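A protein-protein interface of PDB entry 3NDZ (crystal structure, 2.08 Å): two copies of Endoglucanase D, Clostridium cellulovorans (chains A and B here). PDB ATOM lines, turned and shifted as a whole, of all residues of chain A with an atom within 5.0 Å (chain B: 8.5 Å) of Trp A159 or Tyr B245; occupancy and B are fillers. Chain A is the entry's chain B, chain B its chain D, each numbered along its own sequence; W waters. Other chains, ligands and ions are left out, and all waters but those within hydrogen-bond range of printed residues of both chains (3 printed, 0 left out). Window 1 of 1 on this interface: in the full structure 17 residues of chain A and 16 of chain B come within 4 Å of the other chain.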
ATOM      1  N   SER A 156      -2.884  24.412  18.899  1.00  0.00           N
ATOM      2  CA  SER A 156      -4.029  24.619  19.772  1.00  0.00           C
ATOM      3  C   SER A 156      -4.886  23.357  19.882  1.00  0.00           C
ATOM      4  O   SER A 156      -5.716  23.234  20.785  1.00  0.00           O
ATOM      5  CB  SER A 156      -4.868  25.806  19.291  1.00  0.00           C
ATOM      6  OG  SER A 156      -5.635  25.478  18.143  1.00  0.00           O
ATOM      7  N   LEU A 157      -4.673  22.417  18.964  1.00  0.00           N
ATOM      8  CA  LEU A 157      -5.473  21.205  18.926  1.00  0.00           C
ATOM      9  C   LEU A 157      -4.704  20.030  19.512  1.00  0.00           C
ATOM     10  O   LEU A 157      -5.235  18.932  19.633  1.00  0.00           O
ATOM     11  CB  LEU A 157      -5.912  20.898  17.490  1.00  0.00           C
ATOM     12  CG  LEU A 157      -6.703  22.012  16.808  1.00  0.00           C
ATOM     13  CD1 LEU A 157      -7.072  21.616  15.374  1.00  0.00           C
ATOM     14  CD2 LEU A 157      -7.942  22.345  17.608  1.00  0.00           C
ATOM     15  N   GLN A 158      -3.455  20.276  19.883  1.00  0.00           N
ATOM     16  CA  GLN A 158      -2.548  19.236  20.371  1.00  0.00           C
ATOM     17  C   GLN A 158      -3.161  18.245  21.374  1.00  0.00           C
ATOM     18  O   GLN A 158      -3.030  17.024  21.224  1.00  0.00           O
ATOM     19  CB  GLN A 158      -1.317  19.899  20.991  1.00  0.00           C
ATOM     20  CG  GLN A 158      -0.553  19.013  21.961  1.00  0.00           C
ATOM     21  CD  GLN A 158       0.721  18.445  21.368  1.00  0.00           C
ATOM     22  OE1 GLN A 158       0.868  18.361  20.147  1.00  0.00           O
ATOM     23  NE2 GLN A 158       1.651  18.047  22.234  1.00  0.00           N
ATOM     24  N   TRP A 159      -3.816  18.770  22.401  1.00  0.00           N
ATOM     25  CA  TRP A 159      -4.362  17.925  23.456  1.00  0.00           C
ATOM     26  C   TRP A 159      -5.877  17.819  23.384  1.00  0.00           C
ATOM     27  O   TRP A 159      -6.543  17.717  24.409  1.00  0.00           O
ATOM     28  CB  TRP A 159      -3.945  18.456  24.826  1.00  0.00           C
ATOM     29  CG  TRP A 159      -2.474  18.454  25.012  1.00  0.00           C
ATOM     30  CD1 TRP A 159      -1.633  19.523  24.918  1.00  0.00           C
ATOM     31  CD2 TRP A 159      -1.652  17.316  25.300  1.00  0.00           C
ATOM     32  NE1 TRP A 159      -0.333  19.120  25.143  1.00  0.00           N
ATOM     33  CE2 TRP A 159      -0.322  17.771  25.380  1.00  0.00           C
ATOM     34  CE3 TRP A 159      -1.915  15.957  25.505  1.00  0.00           C
ATOM     35  CZ2 TRP A 159       0.745  16.916  25.654  1.00  0.00           C
ATOM     36  CZ3 TRP A 159      -0.856  15.109  25.778  1.00  0.00           C
ATOM     37  CH2 TRP A 159       0.460  15.592  25.851  1.00  0.00           C
ATOM     38  N   THR A 160      -6.422  17.861  22.175  1.00  0.00           N
ATOM     39  CA  THR A 160      -7.863  17.727  22.003  1.00  0.00           C
ATOM     40  C   THR A 160      -8.218  16.376  21.398  1.00  0.00           C
ATOM     41  O   THR A 160      -7.338  15.628  20.980  1.00  0.00           O
ATOM     42  CB  THR A 160      -8.431  18.856  21.130  1.00  0.00           C
ATOM     43  OG1 THR A 160      -7.997  18.687  19.771  1.00  0.00           O
ATOM     44  CG2 THR A 160      -7.969  20.210  21.656  1.00  0.00           C
ATOM     45  N   GLY A 161      -9.508  16.063  21.357  1.00  0.00           N
ATOM     46  CA  GLY A 161      -9.966  14.865  20.680  1.00  0.00           C
ATOM     47  C   GLY A 161     -10.380  15.125  19.239  1.00  0.00           C
ATOM     48  O   GLY A 161     -11.093  14.327  18.641  1.00  0.00           O
ATOM     49  N   MET A 203      -8.137   9.633  26.250  1.00  0.00           N
ATOM     50  CA  MET A 203      -9.262  10.425  26.758  1.00  0.00           C
ATOM     51  C   MET A 203     -10.599   9.822  26.289  1.00  0.00           C
ATOM     52  O   MET A 203     -10.647   9.141  25.250  1.00  0.00           O
ATOM     53  CB  MET A 203      -9.144  11.888  26.317  1.00  0.00           C
ATOM     54  CG  MET A 203      -9.643  12.134  24.897  1.00  0.00           C
ATOM     55  SD  MET A 203      -9.511  13.853  24.326  1.00  0.00           S
ATOM     56  CE  MET A 203      -7.799  13.948  23.889  1.00  0.00           C
ATOM     57  N   TYR A 229       0.378  14.494  33.258  1.00  0.00           N
ATOM     58  CA  TYR A 229       1.057  15.433  32.362  1.00  0.00           C
ATOM     59  C   TYR A 229       2.109  16.321  33.042  1.00  0.00           C
ATOM     60  O   TYR A 229       3.260  16.374  32.609  1.00  0.00           O
ATOM     61  CB  TYR A 229       0.034  16.305  31.638  1.00  0.00           C
ATOM     62  CG  TYR A 229       0.655  17.421  30.838  1.00  0.00           C
ATOM     63  CD1 TYR A 229       1.246  17.170  29.608  1.00  0.00           C
ATOM     64  CD2 TYR A 229       0.655  18.726  31.315  1.00  0.00           C
ATOM     65  CE1 TYR A 229       1.823  18.189  28.872  1.00  0.00           C
ATOM     66  CE2 TYR A 229       1.229  19.749  30.591  1.00  0.00           C
ATOM     67  CZ  TYR A 229       1.810  19.479  29.367  1.00  0.00           C
ATOM     68  OH  TYR A 229       2.383  20.498  28.636  1.00  0.00           O
ATOM     69  N   MET A 233       5.771  15.262  31.993  1.00  0.00           N
ATOM     70  CA  MET A 233       6.046  15.855  30.704  1.00  0.00           C
ATOM     71  C   MET A 233       6.356  17.348  30.760  1.00  0.00           C
ATOM     72  O   MET A 233       7.174  17.841  29.986  1.00  0.00           O
ATOM     73  CB  MET A 233       4.853  15.577  29.785  1.00  0.00           C
ATOM     74  CG  MET A 233       5.046  15.970  28.349  1.00  0.00           C
ATOM     75  SD  MET A 233       4.007  14.941  27.295  1.00  0.00           S
ATOM     76  CE  MET A 233       5.253  13.860  26.610  1.00  0.00           C
ATOM     77  N   PRO B 228     -13.969  22.798  34.451  1.00  0.00           N
ATOM     78  CA  PRO B 228     -12.727  22.149  34.879  1.00  0.00           C
ATOM     79  C   PRO B 228     -12.328  22.675  36.245  1.00  0.00           C
ATOM     80  O   PRO B 228     -12.611  23.831  36.560  1.00  0.00           O
ATOM     81  CB  PRO B 228     -11.711  22.628  33.838  1.00  0.00           C
ATOM     82  CG  PRO B 228     -12.227  23.964  33.409  1.00  0.00           C
ATOM     83  CD  PRO B 228     -13.721  23.960  33.574  1.00  0.00           C
ATOM     84  N   PHE B 230      -9.577  23.842  37.803  1.00  0.00           N
ATOM     85  CA  PHE B 230      -8.776  25.041  38.036  1.00  0.00           C
ATOM     86  C   PHE B 230      -9.533  26.338  37.811  1.00  0.00           C
ATOM     87  O   PHE B 230      -9.395  27.286  38.583  1.00  0.00           O
ATOM     88  CB  PHE B 230      -7.489  25.013  37.210  1.00  0.00           C
ATOM     89  CG  PHE B 230      -6.461  24.068  37.748  1.00  0.00           C
ATOM     90  CD1 PHE B 230      -6.178  24.044  39.108  1.00  0.00           C
ATOM     91  CD2 PHE B 230      -5.780  23.202  36.907  1.00  0.00           C
ATOM     92  CE1 PHE B 230      -5.237  23.169  39.620  1.00  0.00           C
ATOM     93  CE2 PHE B 230      -4.833  22.328  37.412  1.00  0.00           C
ATOM     94  CZ  PHE B 230      -4.564  22.311  38.773  1.00  0.00           C
ATOM     95  N   TRP B 241     -11.422  30.877  30.421  1.00  0.00           N
ATOM     96  CA  TRP B 241     -11.960  29.644  29.867  1.00  0.00           C
ATOM     97  C   TRP B 241     -12.501  29.938  28.472  1.00  0.00           C
ATOM     98  O   TRP B 241     -13.223  30.917  28.280  1.00  0.00           O
ATOM     99  CB  TRP B 241     -13.078  29.069  30.760  1.00  0.00           C
ATOM    100  CG  TRP B 241     -13.475  27.661  30.362  1.00  0.00           C
ATOM    101  CD1 TRP B 241     -13.037  26.500  30.930  1.00  0.00           C
ATOM    102  CD2 TRP B 241     -14.356  27.275  29.290  1.00  0.00           C
ATOM    103  NE1 TRP B 241     -13.596  25.419  30.288  1.00  0.00           N
ATOM    104  CE2 TRP B 241     -14.410  25.867  29.282  1.00  0.00           C
ATOM    105  CE3 TRP B 241     -15.115  27.981  28.357  1.00  0.00           C
ATOM    106  CZ2 TRP B 241     -15.190  25.153  28.371  1.00  0.00           C
ATOM    107  CZ3 TRP B 241     -15.879  27.267  27.442  1.00  0.00           C
ATOM    108  CH2 TRP B 241     -15.906  25.866  27.457  1.00  0.00           C
ATOM    109  N   GLY B 242     -12.142  29.108  27.494  1.00  0.00           N
ATOM    110  CA  GLY B 242     -12.686  29.262  26.155  1.00  0.00           C
ATOM    111  C   GLY B 242     -11.886  28.696  24.991  1.00  0.00           C
ATOM    112  O   GLY B 242     -12.328  28.773  23.846  1.00  0.00           O
ATOM    113  N   SER B 243     -10.722  28.124  25.263  1.00  0.00           N
ATOM    114  CA  SER B 243      -9.901  27.578  24.187  1.00  0.00           C
ATOM    115  C   SER B 243     -10.498  26.287  23.628  1.00  0.00           C
ATOM    116  O   SER B 243     -11.392  25.696  24.226  1.00  0.00           O
ATOM    117  CB  SER B 243      -8.487  27.305  24.681  1.00  0.00           C
ATOM    118  OG  SER B 243      -8.503  26.280  25.660  1.00  0.00           O
ATOM    119  N   ASP B 244      -9.999  25.856  22.475  1.00  0.00           N
ATOM    120  CA  ASP B 244     -10.381  24.569  21.923  1.00  0.00           C
ATOM    121  C   ASP B 244     -10.024  23.480  22.915  1.00  0.00           C
ATOM    122  O   ASP B 244     -10.747  22.495  23.045  1.00  0.00           O
ATOM    123  CB  ASP B 244      -9.670  24.312  20.591  1.00  0.00           C
ATOM    124  CG  ASP B 244     -10.212  25.178  19.468  1.00  0.00           C
ATOM    125  OD1 ASP B 244     -11.356  25.663  19.600  1.00  0.00           O
ATOM    126  OD2 ASP B 244      -9.501  25.366  18.459  1.00  0.00           O
ATOM    127  N   TYR B 245      -8.905  23.655  23.612  1.00  0.00           N
ATOM    128  CA  TYR B 245      -8.520  22.689  24.634  1.00  0.00           C
ATOM    129  C   TYR B 245      -9.568  22.612  25.736  1.00  0.00           C
ATOM    130  O   TYR B 245      -9.996  21.529  26.119  1.00  0.00           O
ATOM    131  CB  TYR B 245      -7.172  23.047  25.249  1.00  0.00           C
ATOM    132  CG  TYR B 245      -6.833  22.199  26.451  1.00  0.00           C
ATOM    133  CD1 TYR B 245      -6.469  20.865  26.306  1.00  0.00           C
ATOM    134  CD2 TYR B 245      -6.881  22.731  27.736  1.00  0.00           C
ATOM    135  CE1 TYR B 245      -6.152  20.081  27.408  1.00  0.00           C
ATOM    136  CE2 TYR B 245      -6.575  21.954  28.846  1.00  0.00           C
ATOM    137  CZ  TYR B 245      -6.205  20.634  28.676  1.00  0.00           C
ATOM    138  OH  TYR B 245      -5.896  19.860  29.776  1.00  0.00           O
ATOM    139  N   ASP B 246      -9.961  23.774  26.252  1.00  0.00           N
ATOM    140  CA  ASP B 246     -10.960  23.868  27.312  1.00  0.00           C
ATOM    141  C   ASP B 246     -12.250  23.181  26.887  1.00  0.00           C
ATOM    142  O   ASP B 246     -12.829  22.420  27.650  1.00  0.00           O
ATOM    143  CB  ASP B 246     -11.270  25.339  27.629  1.00  0.00           C
ATOM    144  CG  ASP B 246     -10.138  26.037  28.369  1.00  0.00           C
ATOM    145  OD1 ASP B 246      -9.317  25.353  29.023  1.00  0.00           O
ATOM    146  OD2 ASP B 246     -10.081  27.284  28.299  1.00  0.00           O
ATOM    147  N   LYS B 247     -12.696  23.473  25.666  1.00  0.00           N
ATOM    148  CA  LYS B 247     -13.937  22.921  25.145  1.00  0.00           C
ATOM    149  C   LYS B 247     -13.841  21.412  25.020  1.00  0.00           C
ATOM    150  O   LYS B 247     -14.779  20.692  25.358  1.00  0.00           O
ATOM    151  CB  LYS B 247     -14.268  23.519  23.778  1.00  0.00           C
ATOM    152  CG  LYS B 247     -14.688  24.997  23.804  1.00  0.00           C
ATOM    153  CD  LYS B 247     -15.048  25.459  22.405  1.00  0.00           C
ATOM    154  CE  LYS B 247     -15.063  26.968  22.276  1.00  0.00           C
ATOM    155  NZ  LYS B 247     -16.002  27.597  23.230  1.00  0.00           N
ATOM    156  N   SER B 248     -12.698  20.948  24.522  1.00  0.00           N
ATOM    157  CA  SER B 248     -12.496  19.533  24.263  1.00  0.00           C
ATOM    158  C   SER B 248     -12.375  18.742  25.571  1.00  0.00           C
ATOM    159  O   SER B 248     -12.955  17.662  25.705  1.00  0.00           O
ATOM    160  CB  SER B 248     -11.267  19.329  23.380  1.00  0.00           C
ATOM    161  OG  SER B 248     -10.914  17.961  23.296  1.00  0.00           O
ATOM    162  N   SER B 249     -11.633  19.280  26.534  1.00  0.00           N
ATOM    163  CA  SER B 249     -11.500  18.637  27.840  1.00  0.00           C
ATOM    164  C   SER B 249     -12.857  18.456  28.516  1.00  0.00           C
ATOM    165  O   SER B 249     -13.151  17.402  29.069  1.00  0.00           O
ATOM    166  CB  SER B 249     -10.586  19.455  28.751  1.00  0.00           C
ATOM    167  OG  SER B 249      -9.310  19.589  28.167  1.00  0.00           O
ATOM    168  N   LEU B 250     -13.684  19.495  28.477  1.00  0.00           N
ATOM    169  CA  LEU B 250     -15.002  19.428  29.097  1.00  0.00           C
ATOM    170  C   LEU B 250     -15.910  18.393  28.413  1.00  0.00           C
ATOM    171  O   LEU B 250     -16.584  17.605  29.085  1.00  0.00           O
ATOM    172  CB  LEU B 250     -15.673  20.806  29.087  1.00  0.00           C
ATOM    173  CG  LEU B 250     -16.980  20.866  29.890  1.00  0.00           C
ATOM    174  CD1 LEU B 250     -16.718  20.502  31.341  1.00  0.00           C
ATOM    175  CD2 LEU B 250     -17.619  22.238  29.795  1.00  0.00           C
ATOM    176  N   ASP B 251     -15.934  18.419  27.082  1.00  0.00           N
ATOM    177  CA  ASP B 251     -16.677  17.447  26.289  1.00  0.00           C
ATOM    178  C   ASP B 251     -16.310  16.034  26.725  1.00  0.00           C
ATOM    179  O   ASP B 251     -17.177  15.172  26.874  1.00  0.00           O
ATOM    180  CB  ASP B 251     -16.319  17.571  24.810  1.00  0.00           C
ATOM    181  CG  ASP B 251     -16.979  18.764  24.128  1.00  0.00           C
ATOM    182  OD1 ASP B 251     -17.811  19.450  24.752  1.00  0.00           O
ATOM    183  OD2 ASP B 251     -16.655  19.006  22.947  1.00  0.00           O
ATOM    184  N   SER B 252     -15.012  15.803  26.902  1.00  0.00           N
ATOM    185  CA  SER B 252     -14.514  14.467  27.188  1.00  0.00           C
ATOM    186  C   SER B 252     -14.998  13.990  28.551  1.00  0.00           C
ATOM    187  O   SER B 252     -15.310  12.812  28.723  1.00  0.00           O
ATOM    188  CB  SER B 252     -12.986  14.436  27.131  1.00  0.00           C
ATOM    189  OG  SER B 252     -12.516  13.105  27.010  1.00  0.00           O
ATOM    190  N   TYR B 290     -21.461  27.063  27.387  1.00  0.00           N
ATOM    191  CA  TYR B 290     -20.903  25.885  26.736  1.00  0.00           C
ATOM    192  C   TYR B 290     -21.142  24.614  27.579  1.00  0.00           C
ATOM    193  O   TYR B 290     -21.535  23.575  27.052  1.00  0.00           O
ATOM    194  CB  TYR B 290     -19.406  26.069  26.447  1.00  0.00           C
ATOM    195  CG  TYR B 290     -18.864  24.962  25.572  1.00  0.00           C
ATOM    196  CD1 TYR B 290     -18.914  25.057  24.183  1.00  0.00           C
ATOM    197  CD2 TYR B 290     -18.354  23.797  26.132  1.00  0.00           C
ATOM    198  CE1 TYR B 290     -18.446  24.033  23.382  1.00  0.00           C
ATOM    199  CE2 TYR B 290     -17.887  22.771  25.342  1.00  0.00           C
ATOM    200  CZ  TYR B 290     -17.934  22.886  23.971  1.00  0.00           C
ATOM    201  OH  TYR B 290     -17.467  21.848  23.193  1.00  0.00           O
HETATM  202  O   HOH W   1      -8.676  17.977  25.887  1.00  0.00           O
HETATM  203  O   HOH W   2     -12.282  17.248  20.697  1.00  0.00           O
HETATM  204  O   HOH W   3      -6.516  25.041  22.543  1.00  0.00           O
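Trp A159 touches one residue of chain B.
Tyr B245 touches just these residues of chain A: Trp A159 (3.7 Å) and Thr A160 (3.9 Å).
Of chain B, only Asp B244 (3.9 Å), Tyr B245 (3.9 Å) and Ser B248 (3.3 Å) come within 4 Å of Thr A160.
Of the printed residues of chain B, Leu A157 touches Asp B244 (3.5 Å).
Printed residues of chain B within 4 Å of Met A203: Ser B252 (3.7 Å).
Printed residues of chain A within 4 Å of Ser B252: Met A203 (3.7 Å).
Lys B247 touches none of the printed residues of chain A.
The nearest residue of chain A that does not touch Tyr B245 is Ser A156 (4.3 Å).
The backbone carbonyl oxygen (O) of Leu A157 is in hydrogen-bond range of the side-chain hydroxyl (OG1) of Thr A160, at 2.8 Å.
The side-chain sulfur (SD) of Met A203 sits at hydrogen-bond distance from the backbone NH (N) of Gly A161, 3.7 Å away.
The side-chain hydroxyl of Ser B243 sits close to the backbone NH of Tyr B245 (3.4 Å).
The side-chain hydroxyl of Ser B249 is in hydrogen-bond range of the backbone carbonyl oxygen of Tyr B245 (2.9 Å).
Water W1 lies within hydrogen-bond range of O of Trp A159, OG of Ser B249 and OG of Ser B248.
Water W3 bridges the backbone carbonyl oxygen of Ser A156 (2.6 Å) and the backbone NH of Tyr B245 (3.0 Å).
Water W2 lies within hydrogen-bond range of OG of Ser B248 and N of Gly A161.
Of the 15 printed residues of chain B, 4 touch a printed residue of chain A.
Printed residues of chain B that touch a printed residue of chain A: Asp B244, Tyr B245, Ser B248 and Ser B252.
Hydrophobic or aromatic side chains of chain B that line the printed part of chain A: Tyr B245.
Printed residues of chain A that touch a printed residue of chain B: Ser A156, Leu A157, Trp A159, Thr A160, Gly A161 and Met A203.
Among the printed residues, 8 pairs touch across the chains.
The side-chain hydroxyl (OG) of Ser B248 lies within hydrogen-bond range of the backbone NH (N) of Gly A161.
No position is printed for both chains.
Of the 8 pairs that touch across the chains among the printed residues, none has its exchanged pair printed and touching as well.
Among the printed residues, pairs that only touch across the chains: Thr A160 with Ser B248 (3.3 Å), Leu A157 with Asp B244 (3.5 Å), Met A203 with Ser B252 (3.7 Å), Trp A159 with Tyr B245 (3.7 Å), Thr A160 with Asp B244 (3.9 Å), Ser A156 with Asp B244 (3.9 Å) and Thr A160 with Tyr B245 (3.9 Å).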
